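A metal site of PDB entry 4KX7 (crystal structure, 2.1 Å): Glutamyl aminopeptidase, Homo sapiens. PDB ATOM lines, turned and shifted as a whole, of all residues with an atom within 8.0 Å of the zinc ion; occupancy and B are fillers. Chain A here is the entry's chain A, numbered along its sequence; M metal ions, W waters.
The side-chain carboxylate (OE2) of Glu 341 sits close to the side-chain hydroxyl (OH) of Tyr 404, at 3.5 Å.
OG of Ser 345 is in hydrogen-bond range of O of Glu 341, 2.9 Å away.
A ring nitrogen (ND1) of His 322 sits at hydrogen-bond distance from the backbone carbonyl oxygen (O) of Phe 325.
OE2 of Glu 348 sits at hydrogen-bond distance from ND1 of His 318.
OH of Tyr 404 touches the zinc ion, 3.8 Å away.
Four residues have an atom within 4 Å of the zinc ion: His 318, His 322, Glu 341 and Tyr 404.
The nearest printed residue that does not touch the zinc ion is Ala 344 (4.3 Å).
The zinc ion is bound by the side-chain carboxylate of Glu 341 (2.0 Å), a ring nitrogen (NE2) of His 322 (2.2 Å) and a ring nitrogen (NE2) of His 318 (2.3 Å).
The zinc ion has three donor atoms within binding distance.
Slightly farther from the zinc ion lies water W1 (2.8 Å).
Water W1 lies within hydrogen-bond range of the side-chain carboxylate (OE1) of Glu 285 (2.6 Å) and the side-chain carboxylate (OE1) of Glu 319 (3.0 Å).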
ATOM      1  N   GLU A 148      16.729  -7.208 -30.355  1.00  0.00           N
ATOM      2  CA  GLU A 148      15.860  -8.300 -29.897  1.00  0.00           C
ATOM      3  C   GLU A 148      15.784  -9.470 -30.891  1.00  0.00           C
ATOM      4  O   GLU A 148      15.499  -9.256 -32.062  1.00  0.00           O
ATOM      5  CB  GLU A 148      14.460  -7.792 -29.542  1.00  0.00           C
ATOM      6  CG  GLU A 148      13.611  -8.806 -28.782  1.00  0.00           C
ATOM      7  CD  GLU A 148      12.271  -8.272 -28.291  1.00  0.00           C
ATOM      8  OE1 GLU A 148      11.728  -7.319 -28.900  1.00  0.00           O
ATOM      9  OE2 GLU A 148      11.763  -8.836 -27.301  1.00  0.00           O
ATOM     10  N   ALA A 283       8.731  -3.036 -35.891  1.00  0.00           N
ATOM     11  CA  ALA A 283       9.055  -1.982 -34.944  1.00  0.00           C
ATOM     12  C   ALA A 283       9.684  -2.632 -33.717  1.00  0.00           C
ATOM     13  O   ALA A 283       9.537  -3.843 -33.507  1.00  0.00           O
ATOM     14  CB  ALA A 283       7.803  -1.215 -34.560  1.00  0.00           C
ATOM     15  N   MET A 284      10.384  -1.830 -32.914  1.00  0.00           N
ATOM     16  CA  MET A 284      11.084  -2.326 -31.735  1.00  0.00           C
ATOM     17  C   MET A 284      10.939  -1.362 -30.554  1.00  0.00           C
ATOM     18  O   MET A 284      11.236  -0.180 -30.675  1.00  0.00           O
ATOM     19  CB  MET A 284      12.566  -2.552 -32.062  1.00  0.00           C
ATOM     20  CG  MET A 284      13.360  -3.134 -30.911  1.00  0.00           C
ATOM     21  SD  MET A 284      12.535  -4.576 -30.189  1.00  0.00           S
ATOM     22  CE  MET A 284      13.287  -4.516 -28.555  1.00  0.00           C
ATOM     23  N   GLU A 285      10.506  -1.899 -29.411  1.00  0.00           N
ATOM     24  CA  GLU A 285      10.084  -1.079 -28.262  1.00  0.00           C
ATOM     25  C   GLU A 285      11.216  -0.531 -27.397  1.00  0.00           C
ATOM     26  O   GLU A 285      11.021  -0.315 -26.186  1.00  0.00           O
ATOM     27  CB  GLU A 285       9.139  -1.884 -27.372  1.00  0.00           C
ATOM     28  CG  GLU A 285       9.788  -3.055 -26.652  1.00  0.00           C
ATOM     29  CD  GLU A 285       9.661  -4.363 -27.414  1.00  0.00           C
ATOM     30  OE1 GLU A 285       9.509  -4.328 -28.654  1.00  0.00           O
ATOM     31  OE2 GLU A 285       9.725  -5.431 -26.774  1.00  0.00           O
ATOM     32  N   VAL A 315       0.383  -0.465 -34.413  1.00  0.00           N
ATOM     33  CA  VAL A 315       1.790  -0.722 -34.134  1.00  0.00           C
ATOM     34  C   VAL A 315       2.304   0.300 -33.115  1.00  0.00           C
ATOM     35  O   VAL A 315       3.000  -0.055 -32.168  1.00  0.00           O
ATOM     36  CB  VAL A 315       2.672  -0.755 -35.392  1.00  0.00           C
ATOM     37  CG1 VAL A 315       4.128  -1.013 -35.017  1.00  0.00           C
ATOM     38  CG2 VAL A 315       2.217  -1.845 -36.353  1.00  0.00           C
ATOM     39  N   HIS A 318       0.864  -0.777 -29.886  1.00  0.00           N
ATOM     40  CA  HIS A 318       1.623  -1.984 -29.530  1.00  0.00           C
ATOM     41  C   HIS A 318       2.931  -1.621 -28.836  1.00  0.00           C
ATOM     42  O   HIS A 318       3.211  -2.112 -27.748  1.00  0.00           O
ATOM     43  CB  HIS A 318       1.922  -2.799 -30.802  1.00  0.00           C
ATOM     44  CG  HIS A 318       2.534  -4.139 -30.534  1.00  0.00           C
ATOM     45  ND1 HIS A 318       1.804  -5.304 -30.551  1.00  0.00           N
ATOM     46  CD2 HIS A 318       3.804  -4.493 -30.268  1.00  0.00           C
ATOM     47  CE1 HIS A 318       2.598  -6.326 -30.296  1.00  0.00           C
ATOM     48  NE2 HIS A 318       3.828  -5.858 -30.119  1.00  0.00           N
ATOM     49  N   GLU A 319       3.704  -0.758 -29.484  1.00  0.00           N
ATOM     50  CA  GLU A 319       5.013  -0.337 -28.988  1.00  0.00           C
ATOM     51  C   GLU A 319       4.886   0.405 -27.668  1.00  0.00           C
ATOM     52  O   GLU A 319       5.742   0.290 -26.797  1.00  0.00           O
ATOM     53  CB  GLU A 319       5.730   0.532 -30.027  1.00  0.00           C
ATOM     54  CG  GLU A 319       5.976  -0.154 -31.357  1.00  0.00           C
ATOM     55  CD  GLU A 319       6.559  -1.547 -31.216  1.00  0.00           C
ATOM     56  OE1 GLU A 319       7.581  -1.707 -30.524  1.00  0.00           O
ATOM     57  OE2 GLU A 319       5.989  -2.492 -31.802  1.00  0.00           O
ATOM     58  N   VAL A 321       2.502  -0.166 -25.400  1.00  0.00           N
ATOM     59  CA  VAL A 321       2.182  -1.156 -24.349  1.00  0.00           C
ATOM     60  C   VAL A 321       3.461  -1.682 -23.723  1.00  0.00           C
ATOM     61  O   VAL A 321       3.542  -1.865 -22.511  1.00  0.00           O
ATOM     62  CB  VAL A 321       1.371  -2.360 -24.871  1.00  0.00           C
ATOM     63  CG1 VAL A 321       1.009  -3.293 -23.732  1.00  0.00           C
ATOM     64  CG2 VAL A 321       0.114  -1.906 -25.585  1.00  0.00           C
ATOM     65  N   HIS A 322       4.463  -1.916 -24.570  1.00  0.00           N
ATOM     66  CA  HIS A 322       5.733  -2.467 -24.125  1.00  0.00           C
ATOM     67  C   HIS A 322       6.467  -1.599 -23.104  1.00  0.00           C
ATOM     68  O   HIS A 322       7.241  -2.113 -22.311  1.00  0.00           O
ATOM     69  CB  HIS A 322       6.644  -2.736 -25.295  1.00  0.00           C
ATOM     70  CG  HIS A 322       6.365  -4.027 -26.007  1.00  0.00           C
ATOM     71  ND1 HIS A 322       6.305  -5.244 -25.350  1.00  0.00           N
ATOM     72  CD2 HIS A 322       6.163  -4.306 -27.321  1.00  0.00           C
ATOM     73  CE1 HIS A 322       6.064  -6.203 -26.229  1.00  0.00           C
ATOM     74  NE2 HIS A 322       5.976  -5.657 -27.428  1.00  0.00           N
ATOM     75  N   PHE A 325       4.454  -3.334 -20.260  1.00  0.00           N
ATOM     76  CA  PHE A 325       4.635  -4.781 -20.342  1.00  0.00           C
ATOM     77  C   PHE A 325       5.761  -5.152 -21.299  1.00  0.00           C
ATOM     78  O   PHE A 325       5.594  -5.171 -22.519  1.00  0.00           O
ATOM     79  CB  PHE A 325       3.335  -5.474 -20.719  1.00  0.00           C
ATOM     80  CG  PHE A 325       2.338  -5.504 -19.613  1.00  0.00           C
ATOM     81  CD1 PHE A 325       2.367  -6.521 -18.665  1.00  0.00           C
ATOM     82  CD2 PHE A 325       1.387  -4.494 -19.487  1.00  0.00           C
ATOM     83  CE1 PHE A 325       1.450  -6.546 -17.624  1.00  0.00           C
ATOM     84  CE2 PHE A 325       0.470  -4.518 -18.447  1.00  0.00           C
ATOM     85  CZ  PHE A 325       0.504  -5.545 -17.509  1.00  0.00           C
ATOM     86  N   LEU A 337       7.998 -15.342 -23.259  1.00  0.00           N
ATOM     87  CA  LEU A 337       7.903 -14.211 -24.206  1.00  0.00           C
ATOM     88  C   LEU A 337       6.498 -13.631 -24.354  1.00  0.00           C
ATOM     89  O   LEU A 337       6.341 -12.424 -24.513  1.00  0.00           O
ATOM     90  CB  LEU A 337       8.446 -14.611 -25.585  1.00  0.00           C
ATOM     91  CG  LEU A 337       8.395 -13.552 -26.700  1.00  0.00           C
ATOM     92  CD1 LEU A 337       9.250 -12.328 -26.342  1.00  0.00           C
ATOM     93  CD2 LEU A 337       8.816 -14.133 -28.033  1.00  0.00           C
ATOM     94  N   ASN A 340       5.392 -10.512 -22.732  1.00  0.00           N
ATOM     95  CA  ASN A 340       5.680  -9.289 -23.470  1.00  0.00           C
ATOM     96  C   ASN A 340       4.720  -9.172 -24.643  1.00  0.00           C
ATOM     97  O   ASN A 340       3.948  -8.222 -24.725  1.00  0.00           O
ATOM     98  CB  ASN A 340       7.130  -9.281 -23.985  1.00  0.00           C
ATOM     99  CG  ASN A 340       8.148  -8.876 -22.913  1.00  0.00           C
ATOM    100  OD1 ASN A 340       9.241  -8.403 -23.247  1.00  0.00           O
ATOM    101  ND2 ASN A 340       7.805  -9.078 -21.645  1.00  0.00           N
ATOM    102  N   GLU A 341       4.781 -10.161 -25.535  1.00  0.00           N
ATOM    103  CA  GLU A 341       4.143 -10.061 -26.852  1.00  0.00           C
ATOM    104  C   GLU A 341       2.625 -10.185 -26.859  1.00  0.00           C
ATOM    105  O   GLU A 341       1.948  -9.434 -27.571  1.00  0.00           O
ATOM    106  CB  GLU A 341       4.757 -11.051 -27.849  1.00  0.00           C
ATOM    107  CG  GLU A 341       6.238 -10.837 -28.117  1.00  0.00           C
ATOM    108  CD  GLU A 341       6.612  -9.412 -28.478  1.00  0.00           C
ATOM    109  OE1 GLU A 341       5.718  -8.599 -28.813  1.00  0.00           O
ATOM    110  OE2 GLU A 341       7.815  -9.088 -28.440  1.00  0.00           O
ATOM    111  N   GLY A 342       2.113 -11.137 -26.086  1.00  0.00           N
ATOM    112  CA  GLY A 342       0.666 -11.353 -25.979  1.00  0.00           C
ATOM    113  C   GLY A 342      -0.020 -10.159 -25.353  1.00  0.00           C
ATOM    114  O   GLY A 342      -1.097  -9.756 -25.784  1.00  0.00           O
ATOM    115  N   PHE A 343       0.622  -9.586 -24.333  1.00  0.00           N
ATOM    116  CA  PHE A 343       0.122  -8.402 -23.655  1.00  0.00           C
ATOM    117  C   PHE A 343       0.068  -7.179 -24.563  1.00  0.00           C
ATOM    118  O   PHE A 343      -0.931  -6.457 -24.572  1.00  0.00           O
ATOM    119  CB  PHE A 343       0.942  -8.110 -22.396  1.00  0.00           C
ATOM    120  CG  PHE A 343       0.632  -9.025 -21.255  1.00  0.00           C
ATOM    121  CD1 PHE A 343       0.977 -10.362 -21.310  1.00  0.00           C
ATOM    122  CD2 PHE A 343      -0.030  -8.548 -20.131  1.00  0.00           C
ATOM    123  CE1 PHE A 343       0.680 -11.228 -20.266  1.00  0.00           C
ATOM    124  CE2 PHE A 343      -0.323  -9.394 -19.071  1.00  0.00           C
ATOM    125  CZ  PHE A 343       0.030 -10.739 -19.146  1.00  0.00           C
ATOM    126  N   ALA A 344       1.136  -6.956 -25.332  1.00  0.00           N
ATOM    127  CA  ALA A 344       1.142  -5.889 -26.324  1.00  0.00           C
ATOM    128  C   ALA A 344       0.093  -6.135 -27.408  1.00  0.00           C
ATOM    129  O   ALA A 344      -0.622  -5.212 -27.808  1.00  0.00           O
ATOM    130  CB  ALA A 344       2.528  -5.720 -26.929  1.00  0.00           C
ATOM    131  N   SER A 345      -0.021  -7.385 -27.874  1.00  0.00           N
ATOM    132  CA  SER A 345      -1.026  -7.744 -28.880  1.00  0.00           C
ATOM    133  C   SER A 345      -2.461  -7.599 -28.360  1.00  0.00           C
ATOM    134  O   SER A 345      -3.379  -7.387 -29.155  1.00  0.00           O
ATOM    135  CB  SER A 345      -0.792  -9.156 -29.413  1.00  0.00           C
ATOM    136  OG  SER A 345       0.471  -9.272 -30.052  1.00  0.00           O
ATOM    137  N   GLU A 348      -2.897  -3.334 -27.410  1.00  0.00           N
ATOM    138  CA  GLU A 348      -2.846  -2.507 -28.613  1.00  0.00           C
ATOM    139  C   GLU A 348      -4.258  -2.153 -29.087  1.00  0.00           C
ATOM    140  O   GLU A 348      -4.495  -1.052 -29.553  1.00  0.00           O
ATOM    141  CB  GLU A 348      -2.036  -3.177 -29.737  1.00  0.00           C
ATOM    142  CG  GLU A 348      -2.708  -4.373 -30.386  1.00  0.00           C
ATOM    143  CD  GLU A 348      -1.896  -4.983 -31.502  1.00  0.00           C
ATOM    144  OE1 GLU A 348      -2.511  -5.550 -32.434  1.00  0.00           O
ATOM    145  OE2 GLU A 348      -0.657  -4.927 -31.464  1.00  0.00           O
ATOM    146  N   PHE A 399       8.891 -15.766 -31.701  1.00  0.00           N
ATOM    147  CA  PHE A 399       8.222 -14.509 -32.025  1.00  0.00           C
ATOM    148  C   PHE A 399       7.256 -14.831 -33.162  1.00  0.00           C
ATOM    149  O   PHE A 399       7.516 -14.558 -34.324  1.00  0.00           O
ATOM    150  CB  PHE A 399       9.243 -13.451 -32.449  1.00  0.00           C
ATOM    151  CG  PHE A 399      10.067 -12.915 -31.307  1.00  0.00           C
ATOM    152  CD1 PHE A 399      11.196 -13.597 -30.861  1.00  0.00           C
ATOM    153  CD2 PHE A 399       9.731 -11.706 -30.690  1.00  0.00           C
ATOM    154  CE1 PHE A 399      11.961 -13.102 -29.802  1.00  0.00           C
ATOM    155  CE2 PHE A 399      10.490 -11.211 -29.645  1.00  0.00           C
ATOM    156  CZ  PHE A 399      11.607 -11.904 -29.194  1.00  0.00           C
ATOM    157  N   TYR A 404       2.146 -14.021 -29.974  1.00  0.00           N
ATOM    158  CA  TYR A 404       1.362 -12.806 -30.220  1.00  0.00           C
ATOM    159  C   TYR A 404      -0.157 -13.065 -30.192  1.00  0.00           C
ATOM    160  O   TYR A 404      -0.858 -12.541 -29.326  1.00  0.00           O
ATOM    161  CB  TYR A 404       1.740 -12.168 -31.567  1.00  0.00           C
ATOM    162  CG  TYR A 404       3.090 -11.464 -31.603  1.00  0.00           C
ATOM    163  CD1 TYR A 404       4.287 -12.198 -31.626  1.00  0.00           C
ATOM    164  CD2 TYR A 404       3.171 -10.074 -31.642  1.00  0.00           C
ATOM    165  CE1 TYR A 404       5.526 -11.548 -31.670  1.00  0.00           C
ATOM    166  CE2 TYR A 404       4.400  -9.416 -31.690  1.00  0.00           C
ATOM    167  CZ  TYR A 404       5.563 -10.165 -31.705  1.00  0.00           C
ATOM    168  OH  TYR A 404       6.779  -9.508 -31.748  1.00  0.00           O
HETATM  169 ZN    ZN M   1       5.901  -6.645 -29.385  1.00  0.00          ZN
HETATM  170  O   HOH W   1       7.666  -4.747 -30.460  1.00  0.00           O
HETATM  171  O   HOH W   2       7.778  -7.198 -31.694  1.00  0.00           O
